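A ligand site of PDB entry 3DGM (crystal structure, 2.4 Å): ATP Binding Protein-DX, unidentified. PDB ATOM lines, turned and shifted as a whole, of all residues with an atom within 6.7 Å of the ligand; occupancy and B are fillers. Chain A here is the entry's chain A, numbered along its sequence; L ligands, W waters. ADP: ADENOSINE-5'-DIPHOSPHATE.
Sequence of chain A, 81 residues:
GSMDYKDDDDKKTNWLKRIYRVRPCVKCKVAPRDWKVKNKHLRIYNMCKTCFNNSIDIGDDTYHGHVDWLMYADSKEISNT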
ATOM      1  N   VAL A  26      -4.967  -0.384 -17.889  1.00  0.00           N
ATOM      2  CA  VAL A  26      -4.037  -0.201 -16.742  1.00  0.00           C
ATOM      3  C   VAL A  26      -3.582   1.259 -16.531  1.00  0.00           C
ATOM      4  O   VAL A  26      -2.994   1.576 -15.489  1.00  0.00           O
ATOM      5  CB  VAL A  26      -2.728  -1.062 -16.851  1.00  0.00           C
ATOM      6  CG1 VAL A  26      -3.019  -2.589 -16.791  1.00  0.00           C
ATOM      7  CG2 VAL A  26      -1.933  -0.677 -18.095  1.00  0.00           C
ATOM      8  N   ARG A  33      -9.947  -2.401 -22.257  1.00  0.00           N
ATOM      9  CA  ARG A  33      -8.702  -2.668 -22.986  1.00  0.00           C
ATOM     10  C   ARG A  33      -8.880  -2.939 -24.512  1.00  0.00           C
ATOM     11  O   ARG A  33      -9.889  -3.508 -24.961  1.00  0.00           O
ATOM     12  CB  ARG A  33      -7.985  -3.840 -22.322  1.00  0.00           C
ATOM     13  CG  ARG A  33      -7.383  -3.494 -20.985  1.00  0.00           C
ATOM     14  CD  ARG A  33      -6.884  -4.723 -20.266  1.00  0.00           C
ATOM     15  NE  ARG A  33      -6.778  -4.383 -18.856  1.00  0.00           N
ATOM     16  CZ  ARG A  33      -5.953  -4.954 -17.980  1.00  0.00           C
ATOM     17  NH1 ARG A  33      -5.109  -5.922 -18.335  1.00  0.00           N
ATOM     18  NH2 ARG A  33      -5.956  -4.512 -16.722  1.00  0.00           N
ATOM     19  N   ASP A  34      -7.879  -2.538 -25.298  1.00  0.00           N
ATOM     20  CA  ASP A  34      -7.769  -3.021 -26.663  1.00  0.00           C
ATOM     21  C   ASP A  34      -7.495  -4.518 -26.639  1.00  0.00           C
ATOM     22  O   ASP A  34      -7.042  -5.050 -25.610  1.00  0.00           O
ATOM     23  CB  ASP A  34      -6.660  -2.280 -27.458  1.00  0.00           C
ATOM     24  CG  ASP A  34      -6.766  -2.518 -28.967  1.00  0.00           C
ATOM     25  OD1 ASP A  34      -7.879  -2.846 -29.484  1.00  0.00           O
ATOM     26  OD2 ASP A  34      -5.743  -2.363 -29.653  1.00  0.00           O
ATOM     27  N   TRP A  35      -7.777  -5.185 -27.757  1.00  0.00           N
ATOM     28  CA  TRP A  35      -7.745  -6.642 -27.862  1.00  0.00           C
ATOM     29  C   TRP A  35      -7.708  -7.019 -29.322  1.00  0.00           C
ATOM     30  O   TRP A  35      -8.097  -6.212 -30.192  1.00  0.00           O
ATOM     31  CB  TRP A  35      -8.964  -7.303 -27.155  1.00  0.00           C
ATOM     32  CG  TRP A  35     -10.267  -6.863 -27.786  1.00  0.00           C
ATOM     33  CD1 TRP A  35     -10.991  -5.716 -27.506  1.00  0.00           C
ATOM     34  CD2 TRP A  35     -10.972  -7.520 -28.855  1.00  0.00           C
ATOM     35  NE1 TRP A  35     -12.097  -5.639 -28.342  1.00  0.00           N
ATOM     36  CE2 TRP A  35     -12.106  -6.732 -29.170  1.00  0.00           C
ATOM     37  CE3 TRP A  35     -10.731  -8.690 -29.594  1.00  0.00           C
ATOM     38  CZ2 TRP A  35     -13.009  -7.108 -30.173  1.00  0.00           C
ATOM     39  CZ3 TRP A  35     -11.658  -9.065 -30.596  1.00  0.00           C
ATOM     40  CH2 TRP A  35     -12.762  -8.268 -30.877  1.00  0.00           C
ATOM     41  N   LYS A  36      -7.264  -8.239 -29.603  1.00  0.00           N
ATOM     42  CA  LYS A  36      -7.391  -8.860 -30.940  1.00  0.00           C
ATOM     43  C   LYS A  36      -7.484 -10.378 -30.856  1.00  0.00           C
ATOM     44  O   LYS A  36      -7.136 -10.994 -29.813  1.00  0.00           O
ATOM     45  CB  LYS A  36      -6.290  -8.389 -31.925  1.00  0.00           C
ATOM     46  CG  LYS A  36      -4.919  -8.900 -31.599  1.00  0.00           C
ATOM     47  CD  LYS A  36      -3.952  -8.782 -32.769  1.00  0.00           C
ATOM     48  CE  LYS A  36      -2.797  -9.836 -32.569  1.00  0.00           C
ATOM     49  NZ  LYS A  36      -1.518  -9.586 -33.371  1.00  0.00           N
ATOM     50  N   LYS A  38      -6.113 -13.859 -32.247  1.00  0.00           N
ATOM     51  CA  LYS A  38      -4.775 -14.298 -32.634  1.00  0.00           C
ATOM     52  C   LYS A  38      -4.892 -15.833 -32.710  1.00  0.00           C
ATOM     53  O   LYS A  38      -4.656 -16.517 -31.720  1.00  0.00           O
ATOM     54  CB  LYS A  38      -3.793 -13.795 -31.538  1.00  0.00           C
ATOM     55  CG  LYS A  38      -2.416 -14.460 -31.400  1.00  0.00           C
ATOM     56  CD  LYS A  38      -1.271 -13.571 -31.894  1.00  0.00           C
ATOM     57  CE  LYS A  38       0.022 -14.394 -31.827  1.00  0.00           C
ATOM     58  NZ  LYS A  38       1.119 -13.846 -32.687  1.00  0.00           N
ATOM     59  N   ARG A  43      -6.086 -12.070 -27.375  1.00  0.00           N
ATOM     60  CA  ARG A  43      -5.045 -11.237 -26.822  1.00  0.00           C
ATOM     61  C   ARG A  43      -5.710  -9.984 -26.220  1.00  0.00           C
ATOM     62  O   ARG A  43      -6.347  -9.188 -26.952  1.00  0.00           O
ATOM     63  CB  ARG A  43      -4.066 -10.824 -27.908  1.00  0.00           C
ATOM     64  CG  ARG A  43      -2.994  -9.872 -27.432  1.00  0.00           C
ATOM     65  CD  ARG A  43      -1.828  -9.869 -28.424  1.00  0.00           C
ATOM     66  NE  ARG A  43      -1.092 -11.107 -28.277  1.00  0.00           N
ATOM     67  CZ  ARG A  43       0.022 -11.435 -28.927  1.00  0.00           C
ATOM     68  NH1 ARG A  43       0.587 -10.596 -29.810  1.00  0.00           N
ATOM     69  NH2 ARG A  43       0.581 -12.607 -28.680  1.00  0.00           N
ATOM     70  N   TYR A  45      -4.768  -6.638 -24.581  1.00  0.00           N
ATOM     71  CA  TYR A  45      -3.646  -5.707 -24.332  1.00  0.00           C
ATOM     72  C   TYR A  45      -3.893  -5.013 -23.005  1.00  0.00           C
ATOM     73  O   TYR A  45      -5.012  -4.946 -22.566  1.00  0.00           O
ATOM     74  CB  TYR A  45      -3.586  -4.647 -25.440  1.00  0.00           C
ATOM     75  CG  TYR A  45      -3.261  -5.233 -26.771  1.00  0.00           C
ATOM     76  CD1 TYR A  45      -1.974  -5.758 -27.037  1.00  0.00           C
ATOM     77  CD2 TYR A  45      -4.224  -5.302 -27.762  1.00  0.00           C
ATOM     78  CE1 TYR A  45      -1.660  -6.321 -28.277  1.00  0.00           C
ATOM     79  CE2 TYR A  45      -3.928  -5.864 -29.019  1.00  0.00           C
ATOM     80  CZ  TYR A  45      -2.642  -6.362 -29.254  1.00  0.00           C
ATOM     81  OH  TYR A  45      -2.356  -6.892 -30.495  1.00  0.00           O
ATOM     82  N   ASN A  46      -2.834  -4.512 -22.384  1.00  0.00           N
ATOM     83  CA  ASN A  46      -2.969  -3.822 -21.098  1.00  0.00           C
ATOM     84  C   ASN A  46      -3.716  -2.493 -21.143  1.00  0.00           C
ATOM     85  O   ASN A  46      -4.297  -2.096 -20.134  1.00  0.00           O
ATOM     86  CB  ASN A  46      -1.590  -3.634 -20.451  1.00  0.00           C
ATOM     87  CG  ASN A  46      -0.828  -4.954 -20.271  1.00  0.00           C
ATOM     88  OD1 ASN A  46      -1.448  -6.047 -20.211  1.00  0.00           O
ATOM     89  ND2 ASN A  46       0.499  -4.861 -20.137  1.00  0.00           N
ATOM     90  N   MET A  47      -3.668  -1.795 -22.280  1.00  0.00           N
ATOM     91  CA  MET A  47      -4.243  -0.451 -22.397  1.00  0.00           C
ATOM     92  C   MET A  47      -5.377  -0.366 -23.415  1.00  0.00           C
ATOM     93  O   MET A  47      -5.453  -1.196 -24.340  1.00  0.00           O
ATOM     94  CB  MET A  47      -3.179   0.608 -22.743  1.00  0.00           C
ATOM     95  CG  MET A  47      -2.278   0.949 -21.568  1.00  0.00           C
ATOM     96  SD  MET A  47      -1.021   2.193 -21.886  1.00  0.00           S
ATOM     97  CE  MET A  47       0.025   1.331 -23.121  1.00  0.00           C
ATOM     98  N   CYS A  48      -6.263   0.622 -23.217  1.00  0.00           N
ATOM     99  CA  CYS A  48      -7.179   0.975 -24.285  1.00  0.00           C
ATOM    100  C   CYS A  48      -6.344   1.573 -25.475  1.00  0.00           C
ATOM    101  O   CYS A  48      -5.117   1.823 -25.341  1.00  0.00           O
ATOM    102  CB  CYS A  48      -8.275   1.928 -23.804  1.00  0.00           C
ATOM    103  SG  CYS A  48      -7.684   3.571 -23.382  1.00  0.00           S
ATOM    104  N   LYS A  49      -6.972   1.780 -26.619  1.00  0.00           N
ATOM    105  CA  LYS A  49      -6.215   2.212 -27.761  1.00  0.00           C
ATOM    106  C   LYS A  49      -5.728   3.652 -27.548  1.00  0.00           C
ATOM    107  O   LYS A  49      -4.571   3.964 -27.862  1.00  0.00           O
ATOM    108  CB  LYS A  49      -7.021   2.130 -29.055  1.00  0.00           C
ATOM    109  CG  LYS A  49      -6.167   2.341 -30.293  1.00  0.00           C
ATOM    110  CD  LYS A  49      -5.591   0.998 -30.766  1.00  0.00           C
ATOM    111  CE  LYS A  49      -4.270   1.203 -31.433  1.00  0.00           C
ATOM    112  NZ  LYS A  49      -3.872  -0.120 -31.988  1.00  0.00           N
ATOM    113  N   CYS A  51      -4.947   5.230 -24.835  1.00  0.00           N
ATOM    114  CA  CYS A  51      -3.783   5.281 -23.916  1.00  0.00           C
ATOM    115  C   CYS A  51      -2.566   4.666 -24.561  1.00  0.00           C
ATOM    116  O   CYS A  51      -1.456   5.203 -24.394  1.00  0.00           O
ATOM    117  CB  CYS A  51      -4.047   4.597 -22.574  1.00  0.00           C
ATOM    118  SG  CYS A  51      -5.122   5.535 -21.514  1.00  0.00           S
ATOM    119  N   PHE A  52      -2.751   3.582 -25.309  1.00  0.00           N
ATOM    120  CA  PHE A  52      -1.649   2.994 -26.087  1.00  0.00           C
ATOM    121  C   PHE A  52      -0.982   3.967 -27.071  1.00  0.00           C
ATOM    122  O   PHE A  52       0.255   4.166 -27.051  1.00  0.00           O
ATOM    123  CB  PHE A  52      -2.064   1.730 -26.867  1.00  0.00           C
ATOM    124  CG  PHE A  52      -0.929   1.137 -27.631  1.00  0.00           C
ATOM    125  CD1 PHE A  52       0.216   0.677 -26.933  1.00  0.00           C
ATOM    126  CD2 PHE A  52      -0.935   1.115 -29.031  1.00  0.00           C
ATOM    127  CE1 PHE A  52       1.328   0.143 -27.622  1.00  0.00           C
ATOM    128  CE2 PHE A  52       0.183   0.584 -29.771  1.00  0.00           C
ATOM    129  CZ  PHE A  52       1.303   0.095 -29.061  1.00  0.00           C
ATOM    130  N   ASN A  53      -1.793   4.555 -27.942  1.00  0.00           N
ATOM    131  CA  ASN A  53      -1.293   5.567 -28.875  1.00  0.00           C
ATOM    132  C   ASN A  53      -0.572   6.691 -28.165  1.00  0.00           C
ATOM    133  O   ASN A  53       0.523   7.122 -28.593  1.00  0.00           O
ATOM    134  CB  ASN A  53      -2.440   6.151 -29.727  1.00  0.00           C
ATOM    135  CG  ASN A  53      -2.934   5.153 -30.792  1.00  0.00           C
ATOM    136  OD1 ASN A  53      -2.241   4.182 -31.120  1.00  0.00           O
ATOM    137  ND2 ASN A  53      -4.130   5.419 -31.355  1.00  0.00           N
ATOM    138  N   SER A  55       0.908   6.541 -25.202  1.00  0.00           N
ATOM    139  CA  SER A  55       2.211   6.100 -24.636  1.00  0.00           C
ATOM    140  C   SER A  55       3.349   6.149 -25.672  1.00  0.00           C
ATOM    141  O   SER A  55       4.520   6.295 -25.321  1.00  0.00           O
ATOM    142  CB  SER A  55       2.073   4.682 -24.099  1.00  0.00           C
ATOM    143  OG  SER A  55       2.027   3.719 -25.149  1.00  0.00           O
ATOM    144  N   TYR A  63       3.666   0.427 -19.590  1.00  0.00           N
ATOM    145  CA  TYR A  63       2.410  -0.331 -19.616  1.00  0.00           C
ATOM    146  C   TYR A  63       2.165  -1.139 -20.866  1.00  0.00           C
ATOM    147  O   TYR A  63       1.105  -1.713 -20.992  1.00  0.00           O
ATOM    148  CB  TYR A  63       1.209   0.602 -19.358  1.00  0.00           C
ATOM    149  CG  TYR A  63       1.408   1.305 -18.038  1.00  0.00           C
ATOM    150  CD1 TYR A  63       1.211   0.600 -16.842  1.00  0.00           C
ATOM    151  CD2 TYR A  63       1.930   2.595 -18.001  1.00  0.00           C
ATOM    152  CE1 TYR A  63       1.444   1.234 -15.614  1.00  0.00           C
ATOM    153  CE2 TYR A  63       2.189   3.241 -16.764  1.00  0.00           C
ATOM    154  CZ  TYR A  63       1.938   2.543 -15.589  1.00  0.00           C
ATOM    155  OH  TYR A  63       2.218   3.138 -14.374  1.00  0.00           O
ATOM    156  N   HIS A  64       3.120  -1.149 -21.812  1.00  0.00           N
ATOM    157  CA  HIS A  64       3.047  -2.035 -22.982  1.00  0.00           C
ATOM    158  C   HIS A  64       2.963  -3.511 -22.573  1.00  0.00           C
ATOM    159  O   HIS A  64       3.594  -3.925 -21.605  1.00  0.00           O
ATOM    160  CB  HIS A  64       4.251  -1.796 -23.910  1.00  0.00           C
ATOM    161  CG  HIS A  64       4.213  -0.451 -24.569  1.00  0.00           C
ATOM    162  ND1 HIS A  64       4.988  -0.123 -25.658  1.00  0.00           N
ATOM    163  CD2 HIS A  64       3.444   0.639 -24.316  1.00  0.00           C
ATOM    164  CE1 HIS A  64       4.726   1.130 -26.015  1.00  0.00           C
ATOM    165  NE2 HIS A  64       3.788   1.613 -25.224  1.00  0.00           N
ATOM    166  N   GLY A  65       2.186  -4.297 -23.291  1.00  0.00           N
ATOM    167  CA  GLY A  65       2.067  -5.714 -22.962  1.00  0.00           C
ATOM    168  C   GLY A  65       0.631  -6.214 -23.151  1.00  0.00           C
ATOM    169  O   GLY A  65      -0.285  -5.449 -23.486  1.00  0.00           O
ATOM    170  N   HIS A  66       0.453  -7.512 -22.880  1.00  0.00           N
ATOM    171  CA  HIS A  66      -0.795  -8.196 -23.174  1.00  0.00           C
ATOM    172  C   HIS A  66      -0.814  -9.538 -22.430  1.00  0.00           C
ATOM    173  O   HIS A  66       0.198  -9.971 -21.882  1.00  0.00           O
ATOM    174  CB  HIS A  66      -0.929  -8.415 -24.694  1.00  0.00           C
ATOM    175  CG  HIS A  66       0.150  -9.260 -25.271  1.00  0.00           C
ATOM    176  ND1 HIS A  66       1.306  -8.726 -25.806  1.00  0.00           N
ATOM    177  CD2 HIS A  66       0.273 -10.604 -25.386  1.00  0.00           C
ATOM    178  CE1 HIS A  66       2.085  -9.710 -26.218  1.00  0.00           C
ATOM    179  NE2 HIS A  66       1.479 -10.860 -25.969  1.00  0.00           N
HETATM  180  PB  ADP L   1       2.854  -9.103 -32.928  1.00  0.00           P
HETATM  181  O1B ADP L   1       2.887 -10.515 -32.324  1.00  0.00           O
HETATM  182  O2B ADP L   1       4.236  -8.469 -33.258  1.00  0.00           O
HETATM  183  O3B ADP L   1       1.765  -9.016 -34.036  1.00  0.00           O
HETATM  184  PA  ADP L   1       1.241  -7.102 -31.448  1.00  0.00           P
HETATM  185  O1A ADP L   1       0.129  -7.830 -30.752  1.00  0.00           O
HETATM  186  O2A ADP L   1       0.995  -6.317 -32.756  1.00  0.00           O
HETATM  187  O3A ADP L   1       2.503  -8.109 -31.648  1.00  0.00           O
HETATM  188  O5' ADP L   1       1.914  -6.214 -30.311  1.00  0.00           O
HETATM  189  C5' ADP L   1       3.020  -5.349 -30.551  1.00  0.00           C
HETATM  190  C4' ADP L   1       3.571  -4.858 -29.205  1.00  0.00           C
HETATM  191  O4' ADP L   1       2.855  -3.706 -28.739  1.00  0.00           O
HETATM  192  C3' ADP L   1       3.451  -5.835 -28.047  1.00  0.00           C
HETATM  193  O3' ADP L   1       4.513  -5.475 -27.132  1.00  0.00           O
HETATM  194  C2' ADP L   1       2.141  -5.458 -27.411  1.00  0.00           C
HETATM  195  O2' ADP L   1       2.105  -5.914 -26.060  1.00  0.00           O
HETATM  196  C1' ADP L   1       2.226  -3.931 -27.487  1.00  0.00           C
HETATM  197  N9  ADP L   1       0.886  -3.356 -27.545  1.00  0.00           N
HETATM  198  C8  ADP L   1       0.135  -3.296 -28.670  1.00  0.00           C
HETATM  199  N7  ADP L   1      -1.086  -2.742 -28.400  1.00  0.00           N
HETATM  200  C5  ADP L   1      -1.104  -2.447 -27.070  1.00  0.00           C
HETATM  201  C6  ADP L   1      -2.097  -1.854 -26.153  1.00  0.00           C
HETATM  202  N6  ADP L   1      -3.323  -1.447 -26.602  1.00  0.00           N
HETATM  203  N1  ADP L   1      -1.724  -1.722 -24.869  1.00  0.00           N
HETATM  204  C2  ADP L   1      -0.516  -2.101 -24.406  1.00  0.00           C
HETATM  205  N3  ADP L   1       0.419  -2.669 -25.175  1.00  0.00           N
HETATM  206  C4  ADP L   1       0.180  -2.873 -26.501  1.00  0.00           C
HETATM  207  O   HOH W   1       4.780  -7.218 -24.998  1.00  0.00           O
HETATM  208  O   HOH W   2      -1.064  -6.584 -34.196  1.00  0.00           O
HETATM  209  O   HOH W   3       4.816  -1.539 -29.273  1.00  0.00           O
HETATM  210  O   HOH W   4      -3.368  -1.647 -29.518  1.00  0.00           O
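OH of Tyr 45 lies within hydrogen-bond range of O1A of the ligand (2.7 Å). An oxygen (O2') of the ligand is in hydrogen-bond range of a ring nitrogen (ND1) of His 66 (2.9 Å). The guanidinium group (NH1) of Arg 43 is in salt-bridge range of an oxygen (O1A) of the ligand. The backbone NH of Gly 65 lies within hydrogen-bond range of a nitrogen (N3) of the ligand (3.1 Å). The backbone NH (N) of Met 47 is in hydrogen-bond range of a nitrogen (N1) of the ligand, 3.2 Å away. O of Met 47 is in hydrogen-bond range of N6 of the ligand (3.1 Å). NZ of Lys 36 is in salt-bridge range of O3B of the ligand (3.4 Å). NZ of Lys 38 is in salt-bridge range of O1B of the ligand, 3.8 Å away.
The backbone carbonyl oxygen (O) of Asp 34 lies within hydrogen-bond range of the backbone NH (N) of Tyr 45. NH2 of Arg 43 lies close to NE2 of His 66, 3.3 Å away. O of Lys 36 is in hydrogen-bond range of N of Arg 43 (2.9 Å). The backbone carbonyl oxygen (O) of Gly 65 lies within hydrogen-bond range of the backbone NH (N) of Asn 46, at 2.9 Å. The backbone NH (N) of Asp 34 lies within hydrogen-bond range of the backbone carbonyl oxygen (O) of Met 47, at 2.9 Å. The side-chain carboxylate (OD2) of Asp 34 is in salt-bridge range of the side-chain amino group (NZ) of Lys 49, at 3.7 Å. O of Tyr 63 lies within hydrogen-bond range of ND2 of Asn 46 (3.3 Å). The backbone NH (N) of Val 26 is in hydrogen-bond range of the backbone carbonyl oxygen (O) of Asn 46 (2.9 Å).
Asp 34 touches the ligand. Asn 46 touches the ligand (N to N1, 3.9 Å). Cys 48 touches the ligand (O to N6, 3.9 Å). CD1 of Phe 52 touches C5 of the ligand (3.4 Å). Tyr 63 touches the ligand (O to C2, 3.8 Å). CA of His 64 touches N3 of the ligand (3.5 Å). 13 residues have an atom within 4 Å of the ligand: Asp 34, Lys 36, Lys 38, Arg 43, Tyr 45, Asn 46, Met 47, Cys 48, Phe 52, Tyr 63, His 64, Gly 65 and His 66. Along chain A the residues within 4 Å of the ligand span positions 34 to 66. The nearest printed residue that does not touch the ligand is Lys 49 (4.8 Å).
Water W2 lies within hydrogen-bond range of O2A of the ligand and NZ of Lys 36. Water W4 lies within hydrogen-bond range of the side-chain carboxylate of Asp 34 (2.5 Å), a nitrogen (N7) of the ligand (2.8 Å) and the side-chain amino group of Lys 49 (2.9 Å).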
